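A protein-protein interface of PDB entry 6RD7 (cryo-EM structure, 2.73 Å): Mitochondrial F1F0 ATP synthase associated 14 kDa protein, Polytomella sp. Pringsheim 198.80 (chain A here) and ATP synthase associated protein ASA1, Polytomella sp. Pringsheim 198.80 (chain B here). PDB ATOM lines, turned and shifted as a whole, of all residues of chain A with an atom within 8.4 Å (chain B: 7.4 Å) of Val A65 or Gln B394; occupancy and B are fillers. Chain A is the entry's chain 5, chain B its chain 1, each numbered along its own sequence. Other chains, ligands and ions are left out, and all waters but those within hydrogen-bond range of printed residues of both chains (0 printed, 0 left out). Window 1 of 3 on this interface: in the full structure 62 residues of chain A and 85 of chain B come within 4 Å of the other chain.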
ATOM      1  N   PRO A  60     -30.312  -5.119 -21.120  1.00  0.00           N
ATOM      2  CA  PRO A  60     -30.929  -6.449 -21.264  1.00  0.00           C
ATOM      3  C   PRO A  60     -30.281  -7.341 -22.315  1.00  0.00           C
ATOM      4  O   PRO A  60     -30.892  -8.341 -22.694  1.00  0.00           O
ATOM      5  CB  PRO A  60     -32.356  -6.086 -21.682  1.00  0.00           C
ATOM      6  CG  PRO A  60     -32.187  -4.853 -22.494  1.00  0.00           C
ATOM      7  CD  PRO A  60     -30.975  -4.122 -21.978  1.00  0.00           C
ATOM      8  N   SER A  61     -29.073  -7.012 -22.773  1.00  0.00           N
ATOM      9  CA  SER A  61     -28.518  -7.670 -23.947  1.00  0.00           C
ATOM     10  C   SER A  61     -27.885  -9.011 -23.601  1.00  0.00           C
ATOM     11  O   SER A  61     -27.726  -9.870 -24.472  1.00  0.00           O
ATOM     12  CB  SER A  61     -27.486  -6.757 -24.601  1.00  0.00           C
ATOM     13  OG  SER A  61     -28.118  -5.681 -25.265  1.00  0.00           O
ATOM     14  N   TYR A  62     -27.521  -9.212 -22.338  1.00  0.00           N
ATOM     15  CA  TYR A  62     -26.690 -10.361 -21.997  1.00  0.00           C
ATOM     16  C   TYR A  62     -27.512 -11.635 -21.862  1.00  0.00           C
ATOM     17  O   TYR A  62     -27.059 -12.715 -22.253  1.00  0.00           O
ATOM     18  CB  TYR A  62     -25.924 -10.074 -20.714  1.00  0.00           C
ATOM     19  CG  TYR A  62     -25.249  -8.734 -20.739  1.00  0.00           C
ATOM     20  CD1 TYR A  62     -24.187  -8.490 -21.597  1.00  0.00           C
ATOM     21  CD2 TYR A  62     -25.683  -7.710 -19.919  1.00  0.00           C
ATOM     22  CE1 TYR A  62     -23.572  -7.265 -21.628  1.00  0.00           C
ATOM     23  CE2 TYR A  62     -25.075  -6.487 -19.943  1.00  0.00           C
ATOM     24  CZ  TYR A  62     -24.022  -6.268 -20.798  1.00  0.00           C
ATOM     25  OH  TYR A  62     -23.417  -5.040 -20.820  1.00  0.00           O
ATOM     26  N   ASP A  63     -28.718 -11.532 -21.314  1.00  0.00           N
ATOM     27  CA  ASP A  63     -29.595 -12.687 -21.145  1.00  0.00           C
ATOM     28  C   ASP A  63     -30.712 -12.702 -22.179  1.00  0.00           C
ATOM     29  O   ASP A  63     -31.859 -13.028 -21.864  1.00  0.00           O
ATOM     30  CB  ASP A  63     -30.161 -12.730 -19.729  1.00  0.00           C
ATOM     31  CG  ASP A  63     -30.634 -11.377 -19.244  1.00  0.00           C
ATOM     32  OD1 ASP A  63     -30.500 -10.386 -19.990  1.00  0.00           O
ATOM     33  OD2 ASP A  63     -31.142 -11.307 -18.105  1.00  0.00           O
ATOM     34  N   ARG A  64     -30.395 -12.332 -23.422  1.00  0.00           N
ATOM     35  CA  ARG A  64     -31.373 -12.410 -24.503  1.00  0.00           C
ATOM     36  C   ARG A  64     -31.686 -13.855 -24.860  1.00  0.00           C
ATOM     37  O   ARG A  64     -32.779 -14.156 -25.351  1.00  0.00           O
ATOM     38  CB  ARG A  64     -30.853 -11.675 -25.736  1.00  0.00           C
ATOM     39  CG  ARG A  64     -30.883 -10.176 -25.629  1.00  0.00           C
ATOM     40  CD  ARG A  64     -32.287  -9.637 -25.729  1.00  0.00           C
ATOM     41  NE  ARG A  64     -32.273  -8.222 -26.076  1.00  0.00           N
ATOM     42  CZ  ARG A  64     -33.103  -7.322 -25.571  1.00  0.00           C
ATOM     43  NH1 ARG A  64     -34.020  -7.683 -24.687  1.00  0.00           N
ATOM     44  NH2 ARG A  64     -33.013  -6.056 -25.946  1.00  0.00           N
ATOM     45  N   VAL A  65     -30.734 -14.758 -24.616  1.00  0.00           N
ATOM     46  CA  VAL A  65     -30.886 -16.171 -24.955  1.00  0.00           C
ATOM     47  C   VAL A  65     -31.937 -16.840 -24.076  1.00  0.00           C
ATOM     48  O   VAL A  65     -32.530 -17.854 -24.460  1.00  0.00           O
ATOM     49  CB  VAL A  65     -29.505 -16.863 -24.862  1.00  0.00           C
ATOM     50  CG1 VAL A  65     -29.029 -16.981 -23.419  1.00  0.00           C
ATOM     51  CG2 VAL A  65     -29.500 -18.208 -25.559  1.00  0.00           C
ATOM     52  N   LEU A  66     -32.222 -16.261 -22.912  1.00  0.00           N
ATOM     53  CA  LEU A  66     -33.171 -16.874 -21.994  1.00  0.00           C
ATOM     54  C   LEU A  66     -34.601 -16.475 -22.323  1.00  0.00           C
ATOM     55  O   LEU A  66     -35.552 -17.042 -21.774  1.00  0.00           O
ATOM     56  CB  LEU A  66     -32.817 -16.490 -20.566  1.00  0.00           C
ATOM     57  CG  LEU A  66     -31.428 -16.879 -20.073  1.00  0.00           C
ATOM     58  CD1 LEU A  66     -31.256 -16.463 -18.631  1.00  0.00           C
ATOM     59  CD2 LEU A  66     -31.215 -18.367 -20.227  1.00  0.00           C
ATOM     60  N   SER A  67     -34.777 -15.496 -23.204  1.00  0.00           N
ATOM     61  CA  SER A  67     -36.101 -15.126 -23.684  1.00  0.00           C
ATOM     62  C   SER A  67     -36.510 -15.918 -24.913  1.00  0.00           C
ATOM     63  O   SER A  67     -37.654 -15.798 -25.361  1.00  0.00           O
ATOM     64  CB  SER A  67     -36.150 -13.630 -23.990  1.00  0.00           C
ATOM     65  OG  SER A  67     -35.874 -12.867 -22.829  1.00  0.00           O
ATOM     66  N   LEU A  68     -35.605 -16.717 -25.457  1.00  0.00           N
ATOM     67  CA  LEU A  68     -35.814 -17.564 -26.619  1.00  0.00           C
ATOM     68  C   LEU A  68     -36.556 -18.821 -26.179  1.00  0.00           C
ATOM     69  O   LEU A  68     -36.616 -19.096 -24.974  1.00  0.00           O
ATOM     70  CB  LEU A  68     -34.458 -17.891 -27.254  1.00  0.00           C
ATOM     71  CG  LEU A  68     -34.042 -17.085 -28.486  1.00  0.00           C
ATOM     72  CD1 LEU A  68     -33.934 -15.606 -28.177  1.00  0.00           C
ATOM     73  CD2 LEU A  68     -32.724 -17.605 -29.023  1.00  0.00           C
ATOM     74  N   PRO A  69     -37.166 -19.587 -27.092  1.00  0.00           N
ATOM     75  CA  PRO A  69     -37.747 -20.882 -26.700  1.00  0.00           C
ATOM     76  C   PRO A  69     -36.650 -21.854 -26.292  1.00  0.00           C
ATOM     77  O   PRO A  69     -35.665 -22.036 -27.009  1.00  0.00           O
ATOM     78  CB  PRO A  69     -38.470 -21.344 -27.969  1.00  0.00           C
ATOM     79  CG  PRO A  69     -37.833 -20.575 -29.067  1.00  0.00           C
ATOM     80  CD  PRO A  69     -37.543 -19.244 -28.473  1.00  0.00           C
ATOM     81  N   ALA A  70     -36.823 -22.476 -25.127  1.00  0.00           N
ATOM     82  CA  ALA A  70     -35.705 -23.169 -24.504  1.00  0.00           C
ATOM     83  C   ALA A  70     -35.597 -24.617 -24.941  1.00  0.00           C
ATOM     84  O   ALA A  70     -34.666 -25.307 -24.514  1.00  0.00           O
ATOM     85  CB  ALA A  70     -35.823 -23.109 -22.983  1.00  0.00           C
ATOM     86  N   VAL A  71     -36.523 -25.104 -25.775  1.00  0.00           N
ATOM     87  CA  VAL A  71     -36.615 -26.548 -25.955  1.00  0.00           C
ATOM     88  C   VAL A  71     -35.487 -27.057 -26.844  1.00  0.00           C
ATOM     89  O   VAL A  71     -34.512 -27.626 -26.338  1.00  0.00           O
ATOM     90  CB  VAL A  71     -38.003 -26.914 -26.513  1.00  0.00           C
ATOM     91  CG1 VAL A  71     -38.164 -28.412 -26.646  1.00  0.00           C
ATOM     92  CG2 VAL A  71     -39.077 -26.361 -25.607  1.00  0.00           C
ATOM     93  N   SER A  72     -35.613 -26.880 -28.171  1.00  0.00           N
ATOM     94  CA  SER A  72     -34.608 -26.754 -29.238  1.00  0.00           C
ATOM     95  C   SER A  72     -35.368 -26.840 -30.550  1.00  0.00           C
ATOM     96  O   SER A  72     -36.576 -27.071 -30.544  1.00  0.00           O
ATOM     97  CB  SER A  72     -33.489 -27.803 -29.250  1.00  0.00           C
ATOM     98  OG  SER A  72     -32.801 -27.853 -28.018  1.00  0.00           O
ATOM     99  N   ASN A  74     -33.973 -29.221 -32.289  1.00  0.00           N
ATOM    100  CA  ASN A  74     -33.625 -30.638 -32.296  1.00  0.00           C
ATOM    101  C   ASN A  74     -34.603 -31.464 -31.468  1.00  0.00           C
ATOM    102  O   ASN A  74     -35.034 -32.542 -31.891  1.00  0.00           O
ATOM    103  CB  ASN A  74     -32.203 -30.810 -31.772  1.00  0.00           C
ATOM    104  CG  ASN A  74     -31.894 -32.230 -31.397  1.00  0.00           C
ATOM    105  OD1 ASN A  74     -31.887 -33.113 -32.243  1.00  0.00           O
ATOM    106  ND2 ASN A  74     -31.625 -32.461 -30.120  1.00  0.00           N
ATOM    107  N   VAL B  94     -37.648 -15.377 -15.259  1.00  0.00           N
ATOM    108  CA  VAL B  94     -36.354 -15.934 -15.625  1.00  0.00           C
ATOM    109  C   VAL B  94     -35.319 -15.443 -14.614  1.00  0.00           C
ATOM    110  O   VAL B  94     -35.393 -14.288 -14.167  1.00  0.00           O
ATOM    111  CB  VAL B  94     -36.019 -15.595 -17.092  1.00  0.00           C
ATOM    112  CG1 VAL B  94     -35.881 -14.095 -17.335  1.00  0.00           C
ATOM    113  CG2 VAL B  94     -34.801 -16.327 -17.547  1.00  0.00           C
ATOM    114  N   VAL B 107     -21.166 -17.836 -16.353  1.00  0.00           N
ATOM    115  CA  VAL B 107     -22.427 -17.375 -16.945  1.00  0.00           C
ATOM    116  C   VAL B 107     -22.964 -18.275 -18.065  1.00  0.00           C
ATOM    117  O   VAL B 107     -24.183 -18.511 -18.076  1.00  0.00           O
ATOM    118  CB  VAL B 107     -22.284 -15.910 -17.404  1.00  0.00           C
ATOM    119  CG1 VAL B 107     -23.581 -15.363 -17.973  1.00  0.00           C
ATOM    120  CG2 VAL B 107     -21.862 -15.059 -16.238  1.00  0.00           C
ATOM    121  N   PHE B 111     -26.582 -20.167 -17.898  1.00  0.00           N
ATOM    122  CA  PHE B 111     -27.563 -20.056 -18.974  1.00  0.00           C
ATOM    123  C   PHE B 111     -28.020 -21.426 -19.450  1.00  0.00           C
ATOM    124  O   PHE B 111     -29.218 -21.651 -19.655  1.00  0.00           O
ATOM    125  CB  PHE B 111     -26.972 -19.271 -20.145  1.00  0.00           C
ATOM    126  CG  PHE B 111     -26.948 -17.785 -19.942  1.00  0.00           C
ATOM    127  CD1 PHE B 111     -27.710 -17.186 -18.954  1.00  0.00           C
ATOM    128  CD2 PHE B 111     -26.161 -16.984 -20.751  1.00  0.00           C
ATOM    129  CE1 PHE B 111     -27.684 -15.817 -18.777  1.00  0.00           C
ATOM    130  CE2 PHE B 111     -26.131 -15.619 -20.578  1.00  0.00           C
ATOM    131  CZ  PHE B 111     -26.894 -15.036 -19.590  1.00  0.00           C
ATOM    132  N   ASP B 112     -27.075 -22.357 -19.610  1.00  0.00           N
ATOM    133  CA  ASP B 112     -27.409 -23.710 -20.042  1.00  0.00           C
ATOM    134  C   ASP B 112     -28.244 -24.439 -18.999  1.00  0.00           C
ATOM    135  O   ASP B 112     -29.132 -25.219 -19.350  1.00  0.00           O
ATOM    136  CB  ASP B 112     -26.136 -24.495 -20.341  1.00  0.00           C
ATOM    137  CG  ASP B 112     -25.377 -23.943 -21.523  1.00  0.00           C
ATOM    138  OD1 ASP B 112     -25.980 -23.196 -22.320  1.00  0.00           O
ATOM    139  OD2 ASP B 112     -24.175 -24.251 -21.651  1.00  0.00           O
ATOM    140  N   ILE B 115     -31.827 -22.990 -19.317  1.00  0.00           N
ATOM    141  CA  ILE B 115     -32.422 -23.527 -20.540  1.00  0.00           C
ATOM    142  C   ILE B 115     -32.780 -25.005 -20.371  1.00  0.00           C
ATOM    143  O   ILE B 115     -33.853 -25.444 -20.806  1.00  0.00           O
ATOM    144  CB  ILE B 115     -31.467 -23.288 -21.728  1.00  0.00           C
ATOM    145  CG1 ILE B 115     -31.367 -21.796 -22.060  1.00  0.00           C
ATOM    146  CG2 ILE B 115     -31.890 -24.056 -22.964  1.00  0.00           C
ATOM    147  CD1 ILE B 115     -32.649 -21.170 -22.529  1.00  0.00           C
ATOM    148  N   ARG B 118     -35.919 -25.330 -18.074  1.00  0.00           N
ATOM    149  CA  ARG B 118     -37.127 -24.895 -18.773  1.00  0.00           C
ATOM    150  C   ARG B 118     -37.555 -25.906 -19.835  1.00  0.00           C
ATOM    151  O   ARG B 118     -38.751 -26.217 -19.963  1.00  0.00           O
ATOM    152  CB  ARG B 118     -36.902 -23.518 -19.396  1.00  0.00           C
ATOM    153  CG  ARG B 118     -37.358 -22.365 -18.524  1.00  0.00           C
ATOM    154  CD  ARG B 118     -36.845 -21.035 -19.052  1.00  0.00           C
ATOM    155  NE  ARG B 118     -37.567 -20.596 -20.242  1.00  0.00           N
ATOM    156  CZ  ARG B 118     -36.982 -20.103 -21.329  1.00  0.00           C
ATOM    157  NH1 ARG B 118     -37.715 -19.728 -22.368  1.00  0.00           N
ATOM    158  NH2 ARG B 118     -35.664 -19.984 -21.376  1.00  0.00           N
ATOM    159  N   ASP B 283     -20.247 -14.752 -24.068  1.00  0.00           N
ATOM    160  CA  ASP B 283     -20.865 -15.163 -22.812  1.00  0.00           C
ATOM    161  C   ASP B 283     -19.834 -15.666 -21.814  1.00  0.00           C
ATOM    162  O   ASP B 283     -20.052 -15.567 -20.603  1.00  0.00           O
ATOM    163  CB  ASP B 283     -21.913 -16.243 -23.068  1.00  0.00           C
ATOM    164  CG  ASP B 283     -23.117 -15.719 -23.814  1.00  0.00           C
ATOM    165  OD1 ASP B 283     -23.437 -14.522 -23.663  1.00  0.00           O
ATOM    166  OD2 ASP B 283     -23.747 -16.504 -24.551  1.00  0.00           O
ATOM    167  N   THR B 384     -23.379 -23.403 -36.251  1.00  0.00           N
ATOM    168  CA  THR B 384     -23.382 -23.773 -34.839  1.00  0.00           C
ATOM    169  C   THR B 384     -21.969 -23.778 -34.267  1.00  0.00           C
ATOM    170  O   THR B 384     -21.762 -23.432 -33.098  1.00  0.00           O
ATOM    171  CB  THR B 384     -24.053 -25.138 -34.676  1.00  0.00           C
ATOM    172  OG1 THR B 384     -25.337 -25.106 -35.305  1.00  0.00           O
ATOM    173  CG2 THR B 384     -24.247 -25.494 -33.219  1.00  0.00           C
ATOM    174  N   ARG B 387     -21.306 -20.004 -33.709  1.00  0.00           N
ATOM    175  CA  ARG B 387     -22.113 -19.263 -32.745  1.00  0.00           C
ATOM    176  C   ARG B 387     -21.815 -19.677 -31.314  1.00  0.00           C
ATOM    177  O   ARG B 387     -21.928 -18.862 -30.394  1.00  0.00           O
ATOM    178  CB  ARG B 387     -23.596 -19.457 -33.039  1.00  0.00           C
ATOM    179  CG  ARG B 387     -24.093 -18.664 -34.209  1.00  0.00           C
ATOM    180  CD  ARG B 387     -25.565 -18.888 -34.418  1.00  0.00           C
ATOM    181  NE  ARG B 387     -26.357 -18.305 -33.346  1.00  0.00           N
ATOM    182  CZ  ARG B 387     -27.683 -18.287 -33.333  1.00  0.00           C
ATOM    183  NH1 ARG B 387     -28.332 -17.735 -32.318  1.00  0.00           N
ATOM    184  NH2 ARG B 387     -28.360 -18.826 -34.338  1.00  0.00           N
ATOM    185  N   TYR B 388     -21.471 -20.941 -31.096  1.00  0.00           N
ATOM    186  CA  TYR B 388     -21.271 -21.463 -29.756  1.00  0.00           C
ATOM    187  C   TYR B 388     -19.954 -22.218 -29.689  1.00  0.00           C
ATOM    188  O   TYR B 388     -19.402 -22.644 -30.705  1.00  0.00           O
ATOM    189  CB  TYR B 388     -22.424 -22.380 -29.332  1.00  0.00           C
ATOM    190  CG  TYR B 388     -23.778 -21.896 -29.781  1.00  0.00           C
ATOM    191  CD1 TYR B 388     -24.421 -20.866 -29.114  1.00  0.00           C
ATOM    192  CD2 TYR B 388     -24.409 -22.461 -30.880  1.00  0.00           C
ATOM    193  CE1 TYR B 388     -25.654 -20.414 -29.524  1.00  0.00           C
ATOM    194  CE2 TYR B 388     -25.645 -22.015 -31.296  1.00  0.00           C
ATOM    195  CZ  TYR B 388     -26.262 -20.994 -30.613  1.00  0.00           C
ATOM    196  OH  TYR B 388     -27.493 -20.545 -31.024  1.00  0.00           O
ATOM    197  N   THR B 389     -19.467 -22.358 -28.508  1.00  0.00           N
ATOM    198  CA  THR B 389     -18.319 -23.159 -28.131  1.00  0.00           C
ATOM    199  C   THR B 389     -18.782 -24.561 -27.749  1.00  0.00           C
ATOM    200  O   THR B 389     -19.930 -24.731 -27.332  1.00  0.00           O
ATOM    201  CB  THR B 389     -17.578 -22.507 -26.959  1.00  0.00           C
ATOM    202  OG1 THR B 389     -18.521 -22.082 -25.970  1.00  0.00           O
ATOM    203  CG2 THR B 389     -16.783 -21.312 -27.442  1.00  0.00           C
ATOM    204  N   PRO B 390     -17.921 -25.607 -27.910  1.00  0.00           N
ATOM    205  CA  PRO B 390     -18.368 -26.995 -27.690  1.00  0.00           C
ATOM    206  C   PRO B 390     -18.920 -27.348 -26.314  1.00  0.00           C
ATOM    207  O   PRO B 390     -19.637 -28.343 -26.179  1.00  0.00           O
ATOM    208  CB  PRO B 390     -17.100 -27.802 -27.976  1.00  0.00           C
ATOM    209  CG  PRO B 390     -16.391 -27.005 -28.984  1.00  0.00           C
ATOM    210  CD  PRO B 390     -16.634 -25.572 -28.630  1.00  0.00           C
ATOM    211  N   ASP B 391     -18.621 -26.547 -25.292  1.00  0.00           N
ATOM    212  CA  ASP B 391     -19.156 -26.832 -23.966  1.00  0.00           C
ATOM    213  C   ASP B 391     -20.601 -26.375 -23.826  1.00  0.00           C
ATOM    214  O   ASP B 391     -21.263 -26.718 -22.842  1.00  0.00           O
ATOM    215  CB  ASP B 391     -18.290 -26.169 -22.900  1.00  0.00           C
ATOM    216  CG  ASP B 391     -18.076 -24.697 -23.162  1.00  0.00           C
ATOM    217  OD1 ASP B 391     -17.436 -24.365 -24.180  1.00  0.00           O
ATOM    218  OD2 ASP B 391     -18.550 -23.873 -22.353  1.00  0.00           O
ATOM    219  N   ARG B 392     -21.107 -25.606 -24.786  1.00  0.00           N
ATOM    220  CA  ARG B 392     -22.442 -25.039 -24.656  1.00  0.00           C
ATOM    221  C   ARG B 392     -23.514 -26.084 -24.923  1.00  0.00           C
ATOM    222  O   ARG B 392     -23.284 -27.072 -25.621  1.00  0.00           O
ATOM    223  CB  ARG B 392     -22.619 -23.863 -25.615  1.00  0.00           C
ATOM    224  CG  ARG B 392     -21.709 -22.695 -25.335  1.00  0.00           C
ATOM    225  CD  ARG B 392     -21.858 -22.207 -23.912  1.00  0.00           C
ATOM    226  NE  ARG B 392     -23.194 -21.691 -23.638  1.00  0.00           N
ATOM    227  CZ  ARG B 392     -23.583 -20.447 -23.897  1.00  0.00           C
ATOM    228  NH1 ARG B 392     -22.738 -19.586 -24.441  1.00  0.00           N
ATOM    229  NH2 ARG B 392     -24.818 -20.065 -23.610  1.00  0.00           N
ATOM    230  N   LEU B 393     -24.693 -25.854 -24.342  1.00  0.00           N
ATOM    231  CA  LEU B 393     -25.862 -26.674 -24.639  1.00  0.00           C
ATOM    232  C   LEU B 393     -26.266 -26.550 -26.098  1.00  0.00           C
ATOM    233  O   LEU B 393     -26.581 -27.548 -26.757  1.00  0.00           O
ATOM    234  CB  LEU B 393     -27.019 -26.241 -23.740  1.00  0.00           C
ATOM    235  CG  LEU B 393     -28.386 -26.926 -23.700  1.00  0.00           C
ATOM    236  CD1 LEU B 393     -28.907 -26.711 -22.342  1.00  0.00           C
ATOM    237  CD2 LEU B 393     -29.388 -26.339 -24.670  1.00  0.00           C
ATOM    238  N   GLN B 394     -26.276 -25.322 -26.610  1.00  0.00           N
ATOM    239  CA  GLN B 394     -26.855 -25.072 -27.919  1.00  0.00           C
ATOM    240  C   GLN B 394     -25.917 -25.517 -29.028  1.00  0.00           C
ATOM    241  O   GLN B 394     -26.365 -25.791 -30.145  1.00  0.00           O
ATOM    242  CB  GLN B 394     -27.232 -23.600 -28.030  1.00  0.00           C
ATOM    243  CG  GLN B 394     -28.355 -23.273 -27.068  1.00  0.00           C
ATOM    244  CD  GLN B 394     -28.610 -21.801 -26.895  1.00  0.00           C
ATOM    245  OE1 GLN B 394     -27.769 -20.964 -27.214  1.00  0.00           O
ATOM    246  NE2 GLN B 394     -29.787 -21.472 -26.380  1.00  0.00           N
ATOM    247  N   TYR B 395     -24.626 -25.657 -28.717  1.00  0.00           N
ATOM    248  CA  TYR B 395     -23.713 -26.369 -29.606  1.00  0.00           C
ATOM    249  C   TYR B 395     -24.152 -27.815 -29.796  1.00  0.00           C
ATOM    250  O   TYR B 395     -24.245 -28.295 -30.931  1.00  0.00           O
ATOM    251  CB  TYR B 395     -22.292 -26.315 -29.046  1.00  0.00           C
ATOM    252  CG  TYR B 395     -21.205 -26.868 -29.949  1.00  0.00           C
ATOM    253  CD1 TYR B 395     -20.491 -26.031 -30.791  1.00  0.00           C
ATOM    254  CD2 TYR B 395     -20.867 -28.221 -29.931  1.00  0.00           C
ATOM    255  CE1 TYR B 395     -19.492 -26.523 -31.604  1.00  0.00           C
ATOM    256  CE2 TYR B 395     -19.874 -28.718 -30.741  1.00  0.00           C
ATOM    257  CZ  TYR B 395     -19.190 -27.866 -31.572  1.00  0.00           C
ATOM    258  OH  TYR B 395     -18.195 -28.363 -32.379  1.00  0.00           O
ATOM    259  N   LYS B 396     -24.427 -28.518 -28.693  1.00  0.00           N
ATOM    260  CA  LYS B 396     -24.824 -29.920 -28.769  1.00  0.00           C
ATOM    261  C   LYS B 396     -26.173 -30.078 -29.455  1.00  0.00           C
ATOM    262  O   LYS B 396     -26.362 -30.986 -30.274  1.00  0.00           O
ATOM    263  CB  LYS B 396     -24.866 -30.521 -27.367  1.00  0.00           C
ATOM    264  CG  LYS B 396     -23.608 -30.280 -26.557  1.00  0.00           C
ATOM    265  CD  LYS B 396     -23.825 -30.596 -25.091  1.00  0.00           C
ATOM    266  CE  LYS B 396     -22.671 -30.087 -24.247  1.00  0.00           C
ATOM    267  NZ  LYS B 396     -21.358 -30.454 -24.841  1.00  0.00           N
ATOM    268  N   GLU B 397     -27.108 -29.173 -29.161  1.00  0.00           N
ATOM    269  CA  GLU B 397     -28.422 -29.237 -29.791  1.00  0.00           C
ATOM    270  C   GLU B 397     -28.347 -28.906 -31.277  1.00  0.00           C
ATOM    271  O   GLU B 397     -29.059 -29.509 -32.086  1.00  0.00           O
ATOM    272  CB  GLU B 397     -29.384 -28.302 -29.067  1.00  0.00           C
ATOM    273  CG  GLU B 397     -29.673 -28.732 -27.644  1.00  0.00           C
ATOM    274  CD  GLU B 397     -30.212 -30.148 -27.563  1.00  0.00           C
ATOM    275  OE1 GLU B 397     -31.196 -30.453 -28.265  1.00  0.00           O
ATOM    276  OE2 GLU B 397     -29.652 -30.956 -26.794  1.00  0.00           O
ATOM    277  N   GLY B 398     -27.452 -27.994 -31.665  1.00  0.00           N
ATOM    278  CA  GLY B 398     -27.291 -27.693 -33.075  1.00  0.00           C
ATOM    279  C   GLY B 398     -26.597 -28.805 -33.835  1.00  0.00           C
ATOM    280  O   GLY B 398     -26.896 -29.045 -35.004  1.00  0.00           O
ATOM    281  N   MET B 399     -25.680 -29.516 -33.175  1.00  0.00           N
ATOM    282  CA  MET B 399     -25.040 -30.658 -33.823  1.00  0.00           C
ATOM    283  C   MET B 399     -26.015 -31.818 -33.999  1.00  0.00           C
ATOM    284  O   MET B 399     -26.009 -32.488 -35.039  1.00  0.00           O
ATOM    285  CB  MET B 399     -23.814 -31.101 -33.031  1.00  0.00           C
ATOM    286  CG  MET B 399     -22.667 -30.116 -33.084  1.00  0.00           C
ATOM    287  SD  MET B 399     -22.289 -29.624 -34.766  1.00  0.00           S
ATOM    288  CE  MET B 399     -21.220 -28.220 -34.489  1.00  0.00           C
ATOM    289  N   LYS B 400     -26.878 -32.053 -33.006  1.00  0.00           N
ATOM    290  CA  LYS B 400     -27.903 -33.085 -33.154  1.00  0.00           C
ATOM    291  C   LYS B 400     -28.930 -32.702 -34.217  1.00  0.00           C
ATOM    292  O   LYS B 400     -29.408 -33.561 -34.974  1.00  0.00           O
ATOM    293  CB  LYS B 400     -28.582 -33.339 -31.812  1.00  0.00           C
ATOM    294  CG  LYS B 400     -27.677 -33.955 -30.767  1.00  0.00           C
ATOM    295  CD  LYS B 400     -28.441 -34.250 -29.494  1.00  0.00           C
ATOM    296  CE  LYS B 400     -27.636 -33.866 -28.268  1.00  0.00           C
ATOM    297  NZ  LYS B 400     -28.312 -34.282 -27.011  1.00  0.00           N
ATOM    298  N   ALA B 511     -36.506 -11.712 -31.279  1.00  0.00           N
ATOM    299  CA  ALA B 511     -35.246 -11.338 -30.634  1.00  0.00           C
ATOM    300  C   ALA B 511     -34.611 -10.110 -31.292  1.00  0.00           C
ATOM    301  O   ALA B 511     -34.140  -9.194 -30.598  1.00  0.00           O
ATOM    302  CB  ALA B 511     -34.273 -12.514 -30.660  1.00  0.00           C
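The guanidinium group (NH2) of Arg B118 sits at hydrogen-bond distance from the backbone carbonyl oxygen (O) of Leu A66, at 3.0 Å.
The backbone carbonyl oxygen of Leu A68 sits at hydrogen-bond distance from the guanidinium group of Arg B118, at 2.9 Å.
The side-chain carboxylate (OE1) of Glu B397 sits at hydrogen-bond distance from the side-chain hydroxyl (OG) of Ser A72 (3.1 Å).
The side-chain carboxylate (OE1) of Glu B397 sits at hydrogen-bond distance from the side-chain amide nitrogen (ND2) of Asn A74, at 2.8 Å.
The side-chain carboxylate of Glu B397 is in salt-bridge range of the side-chain amino group of Lys B400.
Among the printed residues, pairs that only touch across the chains: Asn A74 with Lys B400, Val A65 with Gln B394, Ala A70 with Ile B115, Tyr A62 with Phe B111, Ala A70 with Arg B118, Leu A66 with Val B94, Leu A66 with Phe B111, Val A65 with Ile B115, Leu A66 with Ile B115, Asp A63 with Phe B111, Val A65 with Phe B111 and Leu A68 with Ala B511.
Pro A60 touches none of the printed residues of chain B.
Of the printed residues of chain B, Leu A66 touches Val B94 (3.6 Å), Phe B111 (3.6 Å), Ile B115 (3.9 Å) and Arg B118 (3.0 Å).
Printed residues of chain B within 4 Å of Leu A68: Arg B118 and Ala B511.
Val A71 touches none of the printed residues of chain B.
Gln B394 touches one residue of chain A.
The nearest printed residue of chain B that does not touch Asn A74 is Lys B396 (5.5 Å).
Printed residues of chain B that touch a printed residue of chain A: Val B94, Phe B111, Ile B115, Arg B118, Gln B394, Glu B397, Lys B400 and Ala B511.
Hydrophobic or aromatic side chains of chain B within 4 Å of the printed part of chain A: Val B94, Phe B111, Ile B115 and Ala B511.
Of the 14 printed residues of chain A, 8 touch a printed residue of chain B.
Printed residues of chain A that touch a printed residue of chain B: Tyr A62, Asp A63, Val A65, Leu A66, Leu A68, Ala A70, Ser A72 and Asn A74.
Hydrophobic or aromatic side chains of chain A that line the printed part of chain B: Val A65, Leu A66, Leu A68 and Ala A70.
Among the printed residues, 16 pairs touch across the chains.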
